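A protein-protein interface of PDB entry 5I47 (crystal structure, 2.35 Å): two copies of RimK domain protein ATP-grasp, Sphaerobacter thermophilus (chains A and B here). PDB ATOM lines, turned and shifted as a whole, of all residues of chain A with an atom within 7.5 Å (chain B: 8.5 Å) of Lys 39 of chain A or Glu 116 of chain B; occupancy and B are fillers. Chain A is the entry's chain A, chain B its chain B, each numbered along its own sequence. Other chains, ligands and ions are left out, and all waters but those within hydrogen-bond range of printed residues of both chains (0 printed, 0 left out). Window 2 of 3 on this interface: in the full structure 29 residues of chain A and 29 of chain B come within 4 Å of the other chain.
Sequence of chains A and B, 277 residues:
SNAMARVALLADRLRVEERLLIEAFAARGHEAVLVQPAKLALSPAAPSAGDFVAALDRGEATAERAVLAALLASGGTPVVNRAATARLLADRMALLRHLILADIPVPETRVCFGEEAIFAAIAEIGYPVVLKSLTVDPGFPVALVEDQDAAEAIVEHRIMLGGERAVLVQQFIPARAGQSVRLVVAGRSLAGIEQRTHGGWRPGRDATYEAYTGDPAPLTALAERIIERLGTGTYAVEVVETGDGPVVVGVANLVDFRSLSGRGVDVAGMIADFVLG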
ATOM      1  N   VAL A  35      13.330  34.914  28.877  1.00  0.00           N
ATOM      2  CA  VAL A  35      13.126  33.539  28.439  1.00  0.00           C
ATOM      3  C   VAL A  35      12.775  32.727  29.676  1.00  0.00           C
ATOM      4  O   VAL A  35      13.641  32.454  30.518  1.00  0.00           O
ATOM      5  CB  VAL A  35      14.355  32.968  27.722  1.00  0.00           C
ATOM      6  CG1 VAL A  35      14.139  31.504  27.386  1.00  0.00           C
ATOM      7  CG2 VAL A  35      14.649  33.772  26.458  1.00  0.00           C
ATOM      8  N   GLN A  36      11.507  32.357  29.794  1.00  0.00           N
ATOM      9  CA  GLN A  36      11.039  31.633  30.963  1.00  0.00           C
ATOM     10  C   GLN A  36      11.420  30.163  30.842  1.00  0.00           C
ATOM     11  O   GLN A  36      11.037  29.514  29.860  1.00  0.00           O
ATOM     12  CB  GLN A  36       9.534  31.789  31.109  1.00  0.00           C
ATOM     13  CG  GLN A  36       9.076  33.210  30.854  1.00  0.00           C
ATOM     14  CD  GLN A  36       7.584  33.384  31.008  1.00  0.00           C
ATOM     15  OE1 GLN A  36       6.910  33.882  30.102  1.00  0.00           O
ATOM     16  NE2 GLN A  36       7.058  32.987  32.163  1.00  0.00           N
ATOM     17  N   PRO A  37      12.181  29.611  31.788  1.00  0.00           N
ATOM     18  CA  PRO A  37      12.574  28.197  31.686  1.00  0.00           C
ATOM     19  C   PRO A  37      11.401  27.233  31.646  1.00  0.00           C
ATOM     20  O   PRO A  37      11.552  26.124  31.116  1.00  0.00           O
ATOM     21  CB  PRO A  37      13.432  27.987  32.940  1.00  0.00           C
ATOM     22  CG  PRO A  37      13.979  29.351  33.246  1.00  0.00           C
ATOM     23  CD  PRO A  37      12.870  30.300  32.895  1.00  0.00           C
ATOM     24  N   ALA A  38      10.235  27.617  32.174  1.00  0.00           N
ATOM     25  CA  ALA A  38       9.091  26.713  32.197  1.00  0.00           C
ATOM     26  C   ALA A  38       8.652  26.294  30.802  1.00  0.00           C
ATOM     27  O   ALA A  38       8.054  25.227  30.650  1.00  0.00           O
ATOM     28  CB  ALA A  38       7.924  27.360  32.936  1.00  0.00           C
ATOM     29  N   LYS A  39       8.942  27.099  29.785  1.00  0.00           N
ATOM     30  CA  LYS A  39       8.556  26.793  28.415  1.00  0.00           C
ATOM     31  C   LYS A  39       9.639  26.051  27.643  1.00  0.00           C
ATOM     32  O   LYS A  39       9.428  25.729  26.469  1.00  0.00           O
ATOM     33  CB  LYS A  39       8.200  28.082  27.663  1.00  0.00           C
ATOM     34  CG  LYS A  39       7.053  28.881  28.258  1.00  0.00           C
ATOM     35  CD  LYS A  39       6.780  30.134  27.426  1.00  0.00           C
ATOM     36  CE  LYS A  39       5.532  30.869  27.906  1.00  0.00           C
ATOM     37  NZ  LYS A  39       5.270  32.101  27.108  1.00  0.00           N
ATOM     38  N   LEU A  40      10.787  25.782  28.262  1.00  0.00           N
ATOM     39  CA  LEU A  40      11.936  25.214  27.565  1.00  0.00           C
ATOM     40  C   LEU A  40      11.843  23.690  27.575  1.00  0.00           C
ATOM     41  O   LEU A  40      11.948  23.058  28.634  1.00  0.00           O
ATOM     42  CB  LEU A  40      13.240  25.684  28.202  1.00  0.00           C
ATOM     43  CG  LEU A  40      13.558  27.172  28.063  1.00  0.00           C
ATOM     44  CD1 LEU A  40      14.880  27.489  28.735  1.00  0.00           C
ATOM     45  CD2 LEU A  40      13.599  27.564  26.599  1.00  0.00           C
ATOM     46  N   ALA A  41      11.642  23.105  26.397  1.00  0.00           N
ATOM     47  CA  ALA A  41      11.675  21.658  26.191  1.00  0.00           C
ATOM     48  C   ALA A  41      12.821  21.380  25.224  1.00  0.00           C
ATOM     49  O   ALA A  41      12.647  21.470  24.004  1.00  0.00           O
ATOM     50  CB  ALA A  41      10.343  21.142  25.652  1.00  0.00           C
ATOM     51  N   LEU A  42      13.992  21.052  25.765  1.00  0.00           N
ATOM     52  CA  LEU A  42      15.221  20.986  24.988  1.00  0.00           C
ATOM     53  C   LEU A  42      15.490  19.565  24.516  1.00  0.00           C
ATOM     54  O   LEU A  42      15.319  18.604  25.269  1.00  0.00           O
ATOM     55  CB  LEU A  42      16.407  21.490  25.812  1.00  0.00           C
ATOM     56  CG  LEU A  42      16.209  22.863  26.454  1.00  0.00           C
ATOM     57  CD1 LEU A  42      17.369  23.211  27.371  1.00  0.00           C
ATOM     58  CD2 LEU A  42      16.041  23.916  25.392  1.00  0.00           C
ATOM     59  N   VAL B 111      14.130  17.292  27.504  1.00  0.00           N
ATOM     60  CA  VAL B 111      14.398  17.827  28.832  1.00  0.00           C
ATOM     61  C   VAL B 111      13.497  19.041  29.012  1.00  0.00           C
ATOM     62  O   VAL B 111      13.661  20.056  28.326  1.00  0.00           O
ATOM     63  CB  VAL B 111      15.878  18.192  29.010  1.00  0.00           C
ATOM     64  CG1 VAL B 111      16.201  18.383  30.483  1.00  0.00           C
ATOM     65  CG2 VAL B 111      16.767  17.119  28.390  1.00  0.00           C
ATOM     66  N   CYS B 112      12.540  18.936  29.927  1.00  0.00           N
ATOM     67  CA  CYS B 112      11.509  19.948  30.117  1.00  0.00           C
ATOM     68  C   CYS B 112      11.638  20.567  31.500  1.00  0.00           C
ATOM     69  O   CYS B 112      11.616  19.855  32.511  1.00  0.00           O
ATOM     70  CB  CYS B 112      10.117  19.342  29.935  1.00  0.00           C
ATOM     71  SG  CYS B 112       9.942  18.517  28.354  1.00  0.00           S
ATOM     72  N   PHE B 113      11.754  21.894  31.539  1.00  0.00           N
ATOM     73  CA  PHE B 113      11.997  22.618  32.777  1.00  0.00           C
ATOM     74  C   PHE B 113      10.738  23.283  33.326  1.00  0.00           C
ATOM     75  O   PHE B 113      10.832  24.109  34.241  1.00  0.00           O
ATOM     76  CB  PHE B 113      13.122  23.637  32.562  1.00  0.00           C
ATOM     77  CG  PHE B 113      14.459  22.996  32.266  1.00  0.00           C
ATOM     78  CD1 PHE B 113      14.798  22.628  30.973  1.00  0.00           C
ATOM     79  CD2 PHE B 113      15.359  22.733  33.288  1.00  0.00           C
ATOM     80  CE1 PHE B 113      16.016  22.021  30.701  1.00  0.00           C
ATOM     81  CE2 PHE B 113      16.579  22.129  33.023  1.00  0.00           C
ATOM     82  CZ  PHE B 113      16.906  21.772  31.727  1.00  0.00           C
ATOM     83  N   GLY B 114       9.566  22.923  32.810  1.00  0.00           N
ATOM     84  CA  GLY B 114       8.322  23.463  33.334  1.00  0.00           C
ATOM     85  C   GLY B 114       7.124  22.738  32.762  1.00  0.00           C
ATOM     86  O   GLY B 114       7.247  21.898  31.867  1.00  0.00           O
ATOM     87  N   GLU B 115       5.948  23.092  33.294  1.00  0.00           N
ATOM     88  CA  GLU B 115       4.716  22.404  32.915  1.00  0.00           C
ATOM     89  C   GLU B 115       4.409  22.581  31.432  1.00  0.00           C
ATOM     90  O   GLU B 115       4.051  21.620  30.742  1.00  0.00           O
ATOM     91  CB  GLU B 115       3.549  22.910  33.764  1.00  0.00           C
ATOM     92  CG  GLU B 115       2.183  22.542  33.196  1.00  0.00           C
ATOM     93  CD  GLU B 115       1.032  23.140  33.983  1.00  0.00           C
ATOM     94  OE1 GLU B 115       1.288  23.786  35.020  1.00  0.00           O
ATOM     95  OE2 GLU B 115      -0.131  22.959  33.560  1.00  0.00           O
ATOM     96  N   GLU B 116       4.533  23.809  30.928  1.00  0.00           N
ATOM     97  CA  GLU B 116       4.253  24.060  29.518  1.00  0.00           C
ATOM     98  C   GLU B 116       5.181  23.252  28.620  1.00  0.00           C
ATOM     99  O   GLU B 116       4.734  22.639  27.641  1.00  0.00           O
ATOM    100  CB  GLU B 116       4.378  25.555  29.227  1.00  0.00           C
ATOM    101  CG  GLU B 116       4.096  25.952  27.793  1.00  0.00           C
ATOM    102  CD  GLU B 116       3.936  27.451  27.643  1.00  0.00           C
ATOM    103  OE1 GLU B 116       3.587  28.111  28.645  1.00  0.00           O
ATOM    104  OE2 GLU B 116       4.166  27.969  26.529  1.00  0.00           O
ATOM    105  N   ALA B 117       6.478  23.228  28.947  1.00  0.00           N
ATOM    106  CA  ALA B 117       7.434  22.447  28.169  1.00  0.00           C
ATOM    107  C   ALA B 117       7.077  20.966  28.168  1.00  0.00           C
ATOM    108  O   ALA B 117       7.261  20.279  27.155  1.00  0.00           O
ATOM    109  CB  ALA B 117       8.841  22.650  28.717  1.00  0.00           C
ATOM    110  N   ILE B 118       6.581  20.452  29.298  1.00  0.00           N
ATOM    111  CA  ILE B 118       6.198  19.042  29.371  1.00  0.00           C
ATOM    112  C   ILE B 118       5.117  18.736  28.346  1.00  0.00           C
ATOM    113  O   ILE B 118       5.208  17.758  27.594  1.00  0.00           O
ATOM    114  CB  ILE B 118       5.744  18.677  30.795  1.00  0.00           C
ATOM    115  CG1 ILE B 118       6.942  18.648  31.745  1.00  0.00           C
ATOM    116  CG2 ILE B 118       5.010  17.336  30.799  1.00  0.00           C
ATOM    117  CD1 ILE B 118       6.567  18.367  33.182  1.00  0.00           C
ATOM    118  N   PHE B 119       4.083  19.576  28.288  1.00  0.00           N
ATOM    119  CA  PHE B 119       3.034  19.362  27.297  1.00  0.00           C
ATOM    120  C   PHE B 119       3.525  19.673  25.888  1.00  0.00           C
ATOM    121  O   PHE B 119       3.037  19.078  24.918  1.00  0.00           O
ATOM    122  CB  PHE B 119       1.799  20.193  27.648  1.00  0.00           C
ATOM    123  CG  PHE B 119       1.119  19.756  28.918  1.00  0.00           C
ATOM    124  CD1 PHE B 119       0.536  18.503  29.009  1.00  0.00           C
ATOM    125  CD2 PHE B 119       1.061  20.596  30.017  1.00  0.00           C
ATOM    126  CE1 PHE B 119      -0.091  18.092  30.175  1.00  0.00           C
ATOM    127  CE2 PHE B 119       0.437  20.192  31.187  1.00  0.00           C
ATOM    128  CZ  PHE B 119      -0.142  18.935  31.263  1.00  0.00           C
ATOM    129  N   ALA B 120       4.493  20.580  25.751  1.00  0.00           N
ATOM    130  CA  ALA B 120       5.083  20.831  24.441  1.00  0.00           C
ATOM    131  C   ALA B 120       5.819  19.601  23.923  1.00  0.00           C
ATOM    132  O   ALA B 120       5.713  19.259  22.740  1.00  0.00           O
ATOM    133  CB  ALA B 120       6.026  22.033  24.508  1.00  0.00           C
ATOM    134  N   ALA B 121       6.568  18.922  24.796  1.00  0.00           N
ATOM    135  CA  ALA B 121       7.263  17.704  24.393  1.00  0.00           C
ATOM    136  C   ALA B 121       6.291  16.556  24.154  1.00  0.00           C
ATOM    137  O   ALA B 121       6.520  15.727  23.265  1.00  0.00           O
ATOM    138  CB  ALA B 121       8.289  17.315  25.452  1.00  0.00           C
ATOM    139  N   ILE B 122       5.209  16.493  24.933  1.00  0.00           N
ATOM    140  CA  ILE B 122       4.217  15.436  24.757  1.00  0.00           C
ATOM    141  C   ILE B 122       3.523  15.571  23.405  1.00  0.00           C
ATOM    142  O   ILE B 122       3.212  14.571  22.746  1.00  0.00           O
ATOM    143  CB  ILE B 122       3.210  15.460  25.920  1.00  0.00           C
ATOM    144  CG1 ILE B 122       3.844  14.886  27.187  1.00  0.00           C
ATOM    145  CG2 ILE B 122       1.953  14.707  25.557  1.00  0.00           C
ATOM    146  CD1 ILE B 122       2.931  14.918  28.390  1.00  0.00           C
ATOM    147  N   ALA B 123       3.280  16.807  22.966  1.00  0.00           N
ATOM    148  CA  ALA B 123       2.692  17.019  21.648  1.00  0.00           C
ATOM    149  C   ALA B 123       3.642  16.572  20.545  1.00  0.00           C
ATOM    150  O   ALA B 123       3.213  15.965  19.557  1.00  0.00           O
ATOM    151  CB  ALA B 123       2.318  18.489  21.473  1.00  0.00           C
ATOM    152  N   VAL B 155       1.272  15.911  36.330  1.00  0.00           N
ATOM    153  CA  VAL B 155       1.743  17.294  36.387  1.00  0.00           C
ATOM    154  C   VAL B 155       1.105  18.021  37.564  1.00  0.00           C
ATOM    155  O   VAL B 155       1.753  18.833  38.238  1.00  0.00           O
ATOM    156  CB  VAL B 155       1.464  18.013  35.052  1.00  0.00           C
ATOM    157  CG1 VAL B 155       1.772  19.492  35.167  1.00  0.00           C
ATOM    158  CG2 VAL B 155       2.284  17.391  33.932  1.00  0.00           C
ATOM    159  N   ILE B 159       3.308  19.469  40.934  1.00  0.00           N
ATOM    160  CA  ILE B 159       3.145  20.861  41.350  1.00  0.00           C
ATOM    161  C   ILE B 159       2.666  20.925  42.793  1.00  0.00           C
ATOM    162  O   ILE B 159       3.057  21.813  43.561  1.00  0.00           O
ATOM    163  CB  ILE B 159       2.178  21.590  40.395  1.00  0.00           C
ATOM    164  CG1 ILE B 159       2.850  21.854  39.044  1.00  0.00           C
ATOM    165  CG2 ILE B 159       1.674  22.889  41.007  1.00  0.00           C
ATOM    166  CD1 ILE B 159       1.949  22.544  38.036  1.00  0.00           C
ATOM    167  N   VAL B 169      10.733  13.997  29.462  1.00  0.00           N
ATOM    168  CA  VAL B 169       9.589  13.452  28.741  1.00  0.00           C
ATOM    169  C   VAL B 169      10.148  12.501  27.692  1.00  0.00           C
ATOM    170  O   VAL B 169      10.735  12.936  26.695  1.00  0.00           O
ATOM    171  CB  VAL B 169       8.731  14.558  28.111  1.00  0.00           C
ATOM    172  CG1 VAL B 169       7.582  13.953  27.325  1.00  0.00           C
ATOM    173  CG2 VAL B 169       8.198  15.491  29.189  1.00  0.00           C
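The backbone NH (N) of Ala 117 of chain B lies within hydrogen-bond range of the backbone carbonyl oxygen (O) of Ala 38 of chain A. N of Phe 113 of chain B sits at hydrogen-bond distance from O of Leu 40 of chain A (3.1 Å). O of Val 111 of chain B sits at hydrogen-bond distance from N of Leu 42 of chain A (2.8 Å). The backbone carbonyl oxygen (O) of Val 111 of chain B lies close to the backbone carbonyl oxygen (O) of Leu 40 of chain A (3.5 Å).
The side-chain sulfur (SG) of Cys 112 of chain B lies within hydrogen-bond range of the backbone carbonyl oxygen (O) of Ala 117 of chain B, at 3.4 Å.
CB of Phe 113 of chain B touches O of Pro 37 of chain A, 3.3 Å away. Ala 38 of chain A touches Phe 113 of chain B (CA to O, 3.7 Å). O of Ala 38 of chain A touches CA of Gly 114 of chain B, at 3.2 Å. N of Glu 115 of chain B touches O of Ala 38 of chain A, 3.998 Å away. Glu 116 of chain B touches Lys 39 of chain A. C of Lys 39 of chain A touches CB of Ala 117 of chain B (3.7 Å). Leu 40 of chain A touches Ala 117 of chain B (O to CB, 3.1 Å). Ala 41 of chain A touches Val 111 of chain B. Ala 117 of chain B touches Ala 41 of chain A (O to CB, 3.5 Å). Leu 42 of chain A touches Phe 113 of chain B.
Of chain A, only Ala 38 and Lys 39 come within 4 Å of Glu 116 of chain B. Of the printed residues of chain A, Val 111 of chain B touches Leu 40 (3.5 Å), Ala 41 (3.3 Å) and Leu 42 (2.8 Å). Printed residues of chain A within 4 Å of Ala 117 of chain B: Ala 38, Lys 39, Leu 40 and Ala 41. Of the printed residues of chain A, Cys 112 of chain B touches Leu 40 (3.5 Å) and Ala 41 (3.8 Å). Of the printed residues of chain B, Leu 40 of chain A touches Val 111 (3.5 Å), Cys 112 (3.5 Å), Phe 113 (3.1 Å) and Ala 117 (3.1 Å). Printed residues of chain B within 4 Å of Pro 37 of chain A: Phe 113 (3.3 Å). Ile 118 of chain B touches none of the printed residues of chain A. The nearest residue of chain B that does not touch Lys 39 of chain A is Gly 114 of chain B (5.1 Å). The nearest printed residue of chain A that does not touch Gly 114 of chain B is Pro 37 of chain A (4.1 Å).
Of the 16 printed residues of chain B, 7 touch a printed residue of chain A. Printed residues of chain A that touch a printed residue of chain B: Pro 37, Ala 38, Lys 39, Leu 40, Ala 41 and Leu 42. Hydrophobic or aromatic side chains of chain A that line the printed part of chain B: Ala 38, Ala 41 and Leu 42. Among the printed residues, 17 pairs touch across the chains. Among the printed residues, no Asp or Glu carboxylate lies within 4 Å of a Lys or Arg side-chain nitrogen of the other chain.
No position is printed for both chains. Of the 17 pairs that touch across the chains among the printed residues, none has its exchanged pair printed and touching as well.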
